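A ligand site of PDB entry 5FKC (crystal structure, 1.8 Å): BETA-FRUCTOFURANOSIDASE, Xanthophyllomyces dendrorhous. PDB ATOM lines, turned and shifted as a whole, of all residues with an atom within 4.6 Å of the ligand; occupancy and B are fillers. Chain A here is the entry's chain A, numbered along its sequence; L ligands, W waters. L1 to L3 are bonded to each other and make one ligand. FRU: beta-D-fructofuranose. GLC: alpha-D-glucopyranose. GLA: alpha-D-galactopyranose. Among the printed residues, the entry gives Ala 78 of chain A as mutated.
The side-chain amide nitrogen (ND2) of Asn 77 lies within hydrogen-bond range of an oxygen (O6) of FRU L1 (3.0 Å).
The side-chain carboxylate (OD2) of Asp 219 is in hydrogen-bond range of an oxygen (O3) of FRU L1 (2.5 Å).
The side-chain carboxylate of Glu 301 is in hydrogen-bond range of an oxygen (O2) of GLC L2 (2.6 Å).
O2 of GLC L2 sits close to NE2 of His 341, at 3.2 Å.
An oxygen (O6) of FRU L1 sits at hydrogen-bond distance from the side-chain amide oxygen (OE1) of Gln 95 (2.5 Å).
The guanidinium group (NE) of Arg 218 lies within hydrogen-bond range of an oxygen (O3) of FRU L1, 2.9 Å away.
An oxygen (O3) of GLC L2 lies within hydrogen-bond range of the side-chain carboxylate (OE1) of Glu 332 (2.6 Å).
O6 of FRU L1 lies within hydrogen-bond range of NE1 of Trp 103, 2.8 Å away.
The backbone carbonyl oxygen of Leu 168 lies within hydrogen-bond range of an oxygen (O6) of GLA L3 (2.6 Å).
An oxygen (O4) of FRU L1 sits at hydrogen-bond distance from the backbone NH (N) of Asp 144.
The side-chain carboxylate (OE1) of Glu 301 is in hydrogen-bond range of the side-chain hydroxyl (OH) of Tyr 374, 2.6 Å away.
O of Gln 95 is in hydrogen-bond range of N of Asn 77, 2.9 Å away.
NE2 of His 341 lies within hydrogen-bond range of OE1 of Glu 301 (3.1 Å).
The side-chain carboxylate (OE2) of Glu 301 lies within salt-bridge range of the guanidinium group (NH2) of Arg 218, at 2.8 Å.
The backbone NH of Thr 302 is in hydrogen-bond range of the side-chain carboxylate of Asp 219 (2.8 Å).
The guanidinium group of Arg 218 is in salt-bridge range of the side-chain carboxylate of Glu 332, at 3.3 Å.
N of Trp 391 sits at hydrogen-bond distance from O of Tyr 374.
A ring nitrogen (NE2) of His 341 lies within hydrogen-bond range of the side-chain carboxylate of Glu 332 (3.2 Å).
Arg 140 touches the ligand.
Phe 143 touches the ligand.
CD1 of Leu 172 touches O6 of GLA L3 (3.9 Å).
Tyr 374 touches the ligand.
Hydrophobic or aromatic side chains that line the ligand: Trp 103, Phe 143, Leu 168, Leu 172, His 341 and Tyr 374.
The nearest printed residue that does not touch the ligand is Ile 106 (4.02 Å).
Water W7 lies within hydrogen-bond range of an oxygen (O1) of FRU L1 (2.6 Å) and the side-chain amide nitrogen (ND2) of Asn 77 (2.9 Å).
Water W12 bridges O4 of GLC L2 (2.6 Å) and O of Leu 168 (3.3 Å).
Water W6 bridges the guanidinium group of Arg 140 and an oxygen (O5) of GLA L3.
Water W4 lies within hydrogen-bond range of the side-chain carboxylate of Glu 332 (2.7 Å), an oxygen (O3) of GLC L2 (3.0 Å) and the guanidinium group of Arg 218 (3.1 Å).
Water W5 lies within hydrogen-bond range of N of Leu 168, O6 of GLA L3 and NH2 of Arg 140.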
ATOM      1  N   ASN A  77     -30.018 -18.571   7.172  1.00  0.00           N
ATOM      2  CA  ASN A  77     -30.254 -17.148   7.315  1.00  0.00           C
ATOM      3  C   ASN A  77     -31.425 -16.675   6.440  1.00  0.00           C
ATOM      4  O   ASN A  77     -32.550 -17.123   6.657  1.00  0.00           O
ATOM      5  CB  ASN A  77     -28.957 -16.283   7.281  1.00  0.00           C
ATOM      6  CG  ASN A  77     -28.116 -16.440   6.017  1.00  0.00           C
ATOM      7  OD1 ASN A  77     -27.575 -17.498   5.731  1.00  0.00           O
ATOM      8  ND2 ASN A  77     -27.949 -15.332   5.300  1.00  0.00           N
ATOM      9  N   ALA A  78     -31.186 -15.792   5.471  1.00  0.00           N
ATOM     10  CA  ALA A  78     -32.251 -15.051   4.786  1.00  0.00           C
ATOM     11  C   ALA A  78     -33.246 -15.950   4.064  1.00  0.00           C
ATOM     12  O   ALA A  78     -32.845 -16.885   3.379  1.00  0.00           O
ATOM     13  CB  ALA A  78     -31.639 -14.094   3.774  1.00  0.00           C
ATOM     14  N   GLN A  95     -31.434 -19.287   2.740  1.00  0.00           N
ATOM     15  CA  GLN A  95     -29.993 -19.423   2.756  1.00  0.00           C
ATOM     16  C   GLN A  95     -29.655 -20.526   3.767  1.00  0.00           C
ATOM     17  O   GLN A  95     -30.101 -20.438   4.914  1.00  0.00           O
ATOM     18  CB  GLN A  95     -29.337 -18.095   3.154  1.00  0.00           C
ATOM     19  CG  GLN A  95     -29.520 -16.992   2.110  1.00  0.00           C
ATOM     20  CD  GLN A  95     -28.561 -17.134   0.951  1.00  0.00           C
ATOM     21  OE1 GLN A  95     -27.436 -16.681   1.020  1.00  0.00           O
ATOM     22  NE2 GLN A  95     -29.018 -17.783  -0.130  1.00  0.00           N
ATOM     23  N   TRP A 103     -22.086 -19.751   8.592  1.00  0.00           N
ATOM     24  CA  TRP A 103     -22.358 -19.560   7.170  1.00  0.00           C
ATOM     25  C   TRP A 103     -21.258 -20.136   6.283  1.00  0.00           C
ATOM     26  O   TRP A 103     -20.081 -20.111   6.630  1.00  0.00           O
ATOM     27  CB  TRP A 103     -22.494 -18.051   6.942  1.00  0.00           C
ATOM     28  CG  TRP A 103     -22.860 -17.544   5.583  1.00  0.00           C
ATOM     29  CD1 TRP A 103     -24.095 -17.136   5.175  1.00  0.00           C
ATOM     30  CD2 TRP A 103     -21.979 -17.301   4.484  1.00  0.00           C
ATOM     31  NE1 TRP A 103     -24.046 -16.668   3.887  1.00  0.00           N
ATOM     32  CE2 TRP A 103     -22.758 -16.755   3.431  1.00  0.00           C
ATOM     33  CE3 TRP A 103     -20.606 -17.475   4.285  1.00  0.00           C
ATOM     34  CZ2 TRP A 103     -22.214 -16.403   2.206  1.00  0.00           C
ATOM     35  CZ3 TRP A 103     -20.062 -17.122   3.061  1.00  0.00           C
ATOM     36  CH2 TRP A 103     -20.864 -16.579   2.037  1.00  0.00           C
ATOM     37  N   ILE A 106     -23.104 -21.288   0.622  1.00  0.00           N
ATOM     38  CA  ILE A 106     -24.477 -20.963   0.940  1.00  0.00           C
ATOM     39  C   ILE A 106     -25.378 -21.369  -0.231  1.00  0.00           C
ATOM     40  O   ILE A 106     -25.050 -21.163  -1.392  1.00  0.00           O
ATOM     41  CB  ILE A 106     -24.636 -19.508   1.420  1.00  0.00           C
ATOM     42  CG1 ILE A 106     -25.874 -19.374   2.325  1.00  0.00           C
ATOM     43  CG2 ILE A 106     -24.664 -18.525   0.253  1.00  0.00           C
ATOM     44  CD1 ILE A 106     -25.723 -20.001   3.703  1.00  0.00           C
ATOM     45  N   ARG A 140     -18.802 -19.462  -4.823  1.00  0.00           N
ATOM     46  CA  ARG A 140     -18.581 -18.856  -3.521  1.00  0.00           C
ATOM     47  C   ARG A 140     -19.872 -18.729  -2.710  1.00  0.00           C
ATOM     48  O   ARG A 140     -19.822 -18.382  -1.539  1.00  0.00           O
ATOM     49  CB  ARG A 140     -17.888 -17.501  -3.697  1.00  0.00           C
ATOM     50  CG  ARG A 140     -17.347 -16.878  -2.418  1.00  0.00           C
ATOM     51  CD  ARG A 140     -18.168 -15.718  -1.912  1.00  0.00           C
ATOM     52  NE  ARG A 140     -17.435 -15.021  -0.872  1.00  0.00           N
ATOM     53  CZ  ARG A 140     -16.440 -14.156  -1.078  1.00  0.00           C
ATOM     54  NH1 ARG A 140     -16.026 -13.862  -2.321  1.00  0.00           N
ATOM     55  NH2 ARG A 140     -15.835 -13.592  -0.040  1.00  0.00           N
ATOM     56  N   PHE A 143     -26.409 -16.737  -3.229  1.00  0.00           N
ATOM     57  CA  PHE A 143     -26.952 -15.724  -2.318  1.00  0.00           C
ATOM     58  C   PHE A 143     -28.462 -15.545  -2.585  1.00  0.00           C
ATOM     59  O   PHE A 143     -29.065 -16.318  -3.350  1.00  0.00           O
ATOM     60  CB  PHE A 143     -26.194 -14.390  -2.477  1.00  0.00           C
ATOM     61  CG  PHE A 143     -24.878 -14.305  -1.747  1.00  0.00           C
ATOM     62  CD1 PHE A 143     -24.044 -15.402  -1.585  1.00  0.00           C
ATOM     63  CD2 PHE A 143     -24.441 -13.070  -1.278  1.00  0.00           C
ATOM     64  CE1 PHE A 143     -22.814 -15.279  -0.962  1.00  0.00           C
ATOM     65  CE2 PHE A 143     -23.209 -12.940  -0.640  1.00  0.00           C
ATOM     66  CZ  PHE A 143     -22.399 -14.059  -0.472  1.00  0.00           C
ATOM     67  N   ASP A 144     -29.072 -14.572  -1.924  1.00  0.00           N
ATOM     68  CA  ASP A 144     -30.508 -14.289  -2.036  1.00  0.00           C
ATOM     69  C   ASP A 144     -30.935 -14.100  -3.508  1.00  0.00           C
ATOM     70  O   ASP A 144     -30.165 -13.652  -4.355  1.00  0.00           O
ATOM     71  CB  ASP A 144     -30.820 -13.033  -1.198  1.00  0.00           C
ATOM     72  CG  ASP A 144     -32.307 -12.733  -1.050  1.00  0.00           C
ATOM     73  OD1 ASP A 144     -33.178 -13.609  -1.228  1.00  0.00           O
ATOM     74  OD2 ASP A 144     -32.585 -11.548  -0.674  1.00  0.00           O
ATOM     75  N   LEU A 168     -15.517  -9.529  -0.438  1.00  0.00           N
ATOM     76  CA  LEU A 168     -16.942  -9.306  -0.599  1.00  0.00           C
ATOM     77  C   LEU A 168     -17.446  -8.675   0.690  1.00  0.00           C
ATOM     78  O   LEU A 168     -17.368  -9.282   1.770  1.00  0.00           O
ATOM     79  CB  LEU A 168     -17.659 -10.632  -0.884  1.00  0.00           C
ATOM     80  CG  LEU A 168     -19.117 -10.569  -1.396  1.00  0.00           C
ATOM     81  CD1 LEU A 168     -19.534 -11.935  -1.932  1.00  0.00           C
ATOM     82  CD2 LEU A 168     -20.078 -10.086  -0.329  1.00  0.00           C
ATOM     83  N   GLY A 169     -17.943  -7.443   0.600  1.00  0.00           N
ATOM     84  CA  GLY A 169     -18.477  -6.762   1.773  1.00  0.00           C
ATOM     85  C   GLY A 169     -18.450  -5.268   1.666  1.00  0.00           C
ATOM     86  O   GLY A 169     -17.589  -4.701   0.966  1.00  0.00           O
ATOM     87  N   LEU A 172     -15.147  -3.815   2.799  1.00  0.00           N
ATOM     88  CA  LEU A 172     -13.982  -4.310   2.079  1.00  0.00           C
ATOM     89  C   LEU A 172     -13.904  -3.640   0.718  1.00  0.00           C
ATOM     90  O   LEU A 172     -14.766  -2.848   0.358  1.00  0.00           O
ATOM     91  CB  LEU A 172     -14.075  -5.827   1.920  1.00  0.00           C
ATOM     92  CG  LEU A 172     -14.140  -6.611   3.226  1.00  0.00           C
ATOM     93  CD1 LEU A 172     -14.283  -8.101   2.943  1.00  0.00           C
ATOM     94  CD2 LEU A 172     -12.897  -6.343   4.080  1.00  0.00           C
ATOM     95  N   ARG A 218     -26.176  -7.008  -4.822  1.00  0.00           N
ATOM     96  CA  ARG A 218     -26.826  -8.288  -4.569  1.00  0.00           C
ATOM     97  C   ARG A 218     -28.306  -8.198  -4.245  1.00  0.00           C
ATOM     98  O   ARG A 218     -28.874  -7.089  -4.135  1.00  0.00           O
ATOM     99  CB  ARG A 218     -26.076  -9.043  -3.459  1.00  0.00           C
ATOM    100  CG  ARG A 218     -25.974  -8.322  -2.118  1.00  0.00           C
ATOM    101  CD  ARG A 218     -25.487  -9.281  -1.022  1.00  0.00           C
ATOM    102  NE  ARG A 218     -25.101  -8.559   0.191  1.00  0.00           N
ATOM    103  CZ  ARG A 218     -23.974  -7.850   0.344  1.00  0.00           C
ATOM    104  NH1 ARG A 218     -23.068  -7.775  -0.632  1.00  0.00           N
ATOM    105  NH2 ARG A 218     -23.759  -7.188   1.478  1.00  0.00           N
ATOM    106  N   ASP A 219     -28.910  -9.372  -4.112  1.00  0.00           N
ATOM    107  CA  ASP A 219     -30.265  -9.538  -3.611  1.00  0.00           C
ATOM    108  C   ASP A 219     -31.285  -8.991  -4.618  1.00  0.00           C
ATOM    109  O   ASP A 219     -32.094  -8.126  -4.280  1.00  0.00           O
ATOM    110  CB  ASP A 219     -30.426  -8.921  -2.217  1.00  0.00           C
ATOM    111  CG  ASP A 219     -29.401  -9.448  -1.201  1.00  0.00           C
ATOM    112  OD1 ASP A 219     -28.778 -10.499  -1.472  1.00  0.00           O
ATOM    113  OD2 ASP A 219     -29.222  -8.794  -0.155  1.00  0.00           O
ATOM    114  N   GLU A 301     -29.335  -4.108   1.773  1.00  0.00           N
ATOM    115  CA  GLU A 301     -29.450  -5.535   1.471  1.00  0.00           C
ATOM    116  C   GLU A 301     -30.920  -5.928   1.416  1.00  0.00           C
ATOM    117  O   GLU A 301     -31.771  -5.254   2.003  1.00  0.00           O
ATOM    118  CB  GLU A 301     -28.751  -6.368   2.540  1.00  0.00           C
ATOM    119  CG  GLU A 301     -27.266  -6.063   2.706  1.00  0.00           C
ATOM    120  CD  GLU A 301     -26.646  -6.881   3.807  1.00  0.00           C
ATOM    121  OE1 GLU A 301     -27.119  -6.799   4.958  1.00  0.00           O
ATOM    122  OE2 GLU A 301     -25.666  -7.586   3.532  1.00  0.00           O
ATOM    123  N   THR A 302     -31.189  -7.043   0.753  1.00  0.00           N
ATOM    124  CA  THR A 302     -32.509  -7.675   0.664  1.00  0.00           C
ATOM    125  C   THR A 302     -33.657  -6.693   0.469  1.00  0.00           C
ATOM    126  O   THR A 302     -34.709  -6.852   1.074  1.00  0.00           O
ATOM    127  CB  THR A 302     -32.809  -8.622   1.875  1.00  0.00           C
ATOM    128  OG1 THR A 302     -33.111  -7.857   3.051  1.00  0.00           O
ATOM    129  CG2 THR A 302     -31.636  -9.544   2.155  1.00  0.00           C
ATOM    130  N   GLU A 332     -26.765  -1.784   6.592  1.00  0.00           N
ATOM    131  CA  GLU A 332     -25.582  -2.251   7.289  1.00  0.00           C
ATOM    132  C   GLU A 332     -24.742  -1.098   7.832  1.00  0.00           C
ATOM    133  O   GLU A 332     -24.627  -0.054   7.201  1.00  0.00           O
ATOM    134  CB  GLU A 332     -24.671  -3.029   6.355  1.00  0.00           C
ATOM    135  CG  GLU A 332     -25.330  -4.119   5.548  1.00  0.00           C
ATOM    136  CD  GLU A 332     -24.286  -5.085   5.026  1.00  0.00           C
ATOM    137  OE1 GLU A 332     -23.967  -6.035   5.773  1.00  0.00           O
ATOM    138  OE2 GLU A 332     -23.793  -4.878   3.888  1.00  0.00           O
ATOM    139  N   HIS A 341     -27.270  -4.300  11.866  1.00  0.00           N
ATOM    140  CA  HIS A 341     -28.302  -4.484  10.857  1.00  0.00           C
ATOM    141  C   HIS A 341     -29.657  -3.905  11.264  1.00  0.00           C
ATOM    142  O   HIS A 341     -30.199  -4.283  12.308  1.00  0.00           O
ATOM    143  CB  HIS A 341     -28.488  -5.977  10.573  1.00  0.00           C
ATOM    144  CG  HIS A 341     -27.554  -6.532   9.556  1.00  0.00           C
ATOM    145  ND1 HIS A 341     -27.183  -7.865   9.531  1.00  0.00           N
ATOM    146  CD2 HIS A 341     -26.902  -5.953   8.522  1.00  0.00           C
ATOM    147  CE1 HIS A 341     -26.365  -8.083   8.524  1.00  0.00           C
ATOM    148  NE2 HIS A 341     -26.174  -6.940   7.890  1.00  0.00           N
ATOM    149  N   TYR A 374     -33.874  -9.748  10.520  1.00  0.00           N
ATOM    150  CA  TYR A 374     -33.288  -9.091   9.371  1.00  0.00           C
ATOM    151  C   TYR A 374     -33.676  -9.869   8.127  1.00  0.00           C
ATOM    152  O   TYR A 374     -34.225 -10.974   8.236  1.00  0.00           O
ATOM    153  CB  TYR A 374     -31.762  -9.064   9.500  1.00  0.00           C
ATOM    154  CG  TYR A 374     -31.046  -8.114   8.572  1.00  0.00           C
ATOM    155  CD1 TYR A 374     -31.297  -6.742   8.618  1.00  0.00           C
ATOM    156  CD2 TYR A 374     -30.128  -8.589   7.639  1.00  0.00           C
ATOM    157  CE1 TYR A 374     -30.640  -5.863   7.774  1.00  0.00           C
ATOM    158  CE2 TYR A 374     -29.470  -7.721   6.788  1.00  0.00           C
ATOM    159  CZ  TYR A 374     -29.736  -6.357   6.858  1.00  0.00           C
ATOM    160  OH  TYR A 374     -29.074  -5.487   6.031  1.00  0.00           O
ATOM    161  N   TRP A 391     -35.794 -13.335   8.918  1.00  0.00           N
ATOM    162  CA  TRP A 391     -34.955 -14.305   9.610  1.00  0.00           C
ATOM    163  C   TRP A 391     -34.642 -13.791  11.000  1.00  0.00           C
ATOM    164  O   TRP A 391     -34.248 -12.633  11.143  1.00  0.00           O
ATOM    165  CB  TRP A 391     -33.678 -14.505   8.811  1.00  0.00           C
ATOM    166  CG  TRP A 391     -32.427 -14.920   9.541  1.00  0.00           C
ATOM    167  CD1 TRP A 391     -32.196 -16.093  10.165  1.00  0.00           C
ATOM    168  CD2 TRP A 391     -31.214 -14.164   9.612  1.00  0.00           C
ATOM    169  NE1 TRP A 391     -30.910 -16.124  10.651  1.00  0.00           N
ATOM    170  CE2 TRP A 391     -30.283 -14.949  10.323  1.00  0.00           C
ATOM    171  CE3 TRP A 391     -30.818 -12.900   9.152  1.00  0.00           C
ATOM    172  CZ2 TRP A 391     -28.987 -14.515  10.592  1.00  0.00           C
ATOM    173  CZ3 TRP A 391     -29.522 -12.467   9.422  1.00  0.00           C
ATOM    174  CH2 TRP A 391     -28.624 -13.263  10.135  1.00  0.00           C
HETATM  175  C1  FRU L   1     -28.127 -10.442   4.337  1.00  0.00           C
HETATM  176  C2  FRU L   1     -27.243 -11.207   3.348  1.00  0.00           C
HETATM  177  C3  FRU L   1     -27.768 -10.951   1.930  1.00  0.00           C
HETATM  178  C4  FRU L   1     -27.111 -12.089   1.151  1.00  0.00           C
HETATM  179  C5  FRU L   1     -27.202 -13.233   2.169  1.00  0.00           C
HETATM  180  C6  FRU L   1     -26.003 -14.182   2.119  1.00  0.00           C
HETATM  181  O1  FRU L   1     -27.738 -10.606   5.704  1.00  0.00           O
HETATM  182  O2  FRU L   1     -25.869 -10.812   3.442  1.00  0.00           O
HETATM  183  O3  FRU L   1     -27.456  -9.640   1.461  1.00  0.00           O
HETATM  184  O4  FRU L   1     -27.788 -12.424  -0.080  1.00  0.00           O
HETATM  185  O5  FRU L   1     -27.329 -12.624   3.455  1.00  0.00           O
HETATM  186  O6  FRU L   1     -26.273 -15.405   2.837  1.00  0.00           O
HETATM  187  C1  GLC L   2     -25.098 -11.241   4.575  1.00  0.00           C
HETATM  188  C2  GLC L   2     -24.475 -10.042   5.301  1.00  0.00           C
HETATM  189  C3  GLC L   2     -23.398  -9.370   4.455  1.00  0.00           C
HETATM  190  C4  GLC L   2     -22.357 -10.408   4.083  1.00  0.00           C
HETATM  191  C5  GLC L   2     -23.017 -11.613   3.388  1.00  0.00           C
HETATM  192  C6  GLC L   2     -22.006 -12.736   3.201  1.00  0.00           C
HETATM  193  O2  GLC L   2     -25.489  -9.098   5.684  1.00  0.00           O
HETATM  194  O3  GLC L   2     -22.815  -8.290   5.197  1.00  0.00           O
HETATM  195  O4  GLC L   2     -21.377  -9.860   3.208  1.00  0.00           O
HETATM  196  O5  GLC L   2     -24.092 -12.142   4.159  1.00  0.00           O
HETATM  197  O6  GLC L   2     -21.414 -12.978   4.478  1.00  0.00           O
HETATM  198  C1  GLA L   3     -20.444 -14.008   4.532  1.00  0.00           C
HETATM  199  C2  GLA L   3     -20.045 -14.300   5.979  1.00  0.00           C
HETATM  200  C3  GLA L   3     -19.375 -13.076   6.586  1.00  0.00           C
HETATM  201  C4  GLA L   3     -18.180 -12.648   5.724  1.00  0.00           C
HETATM  202  C5  GLA L   3     -18.610 -12.483   4.251  1.00  0.00           C
HETATM  203  C6  GLA L   3     -17.468 -12.229   3.272  1.00  0.00           C
HETATM  204  O2  GLA L   3     -21.201 -14.658   6.727  1.00  0.00           O
HETATM  205  O3  GLA L   3     -18.982 -13.388   7.940  1.00  0.00           O
HETATM  206  O4  GLA L   3     -17.131 -13.624   5.868  1.00  0.00           O
HETATM  207  O5  GLA L   3     -19.300 -13.664   3.779  1.00  0.00           O
HETATM  208  O6  GLA L   3     -16.860 -10.987   3.600  1.00  0.00           O
HETATM  209  O   HOH W   1     -14.623 -13.674   5.080  1.00  0.00           O
HETATM  210  O   HOH W   2     -21.314 -14.960   9.379  1.00  0.00           O
HETATM  211  O   HOH W   3     -23.652 -13.512   6.657  1.00  0.00           O
HETATM  212  O   HOH W   4     -21.529  -6.297   3.398  1.00  0.00           O
HETATM  213  O   HOH W   5     -14.447 -11.282   1.699  1.00  0.00           O
HETATM  214  O   HOH W   6     -17.487 -15.271   2.051  1.00  0.00           O
HETATM  215  O   HOH W   7     -28.831 -12.868   6.458  1.00  0.00           O
HETATM  216  O   HOH W   8     -15.191 -10.398   5.939  1.00  0.00           O
HETATM  217  O   HOH W   9     -17.066 -16.358   5.764  1.00  0.00           O
HETATM  218  O   HOH W  10     -21.596  -9.135   7.432  1.00  0.00           O
HETATM  219  O   HOH W  11     -15.882 -13.969   8.362  1.00  0.00           O
HETATM  220  O   HOH W  12     -19.286  -8.784   4.397  1.00  0.00           O
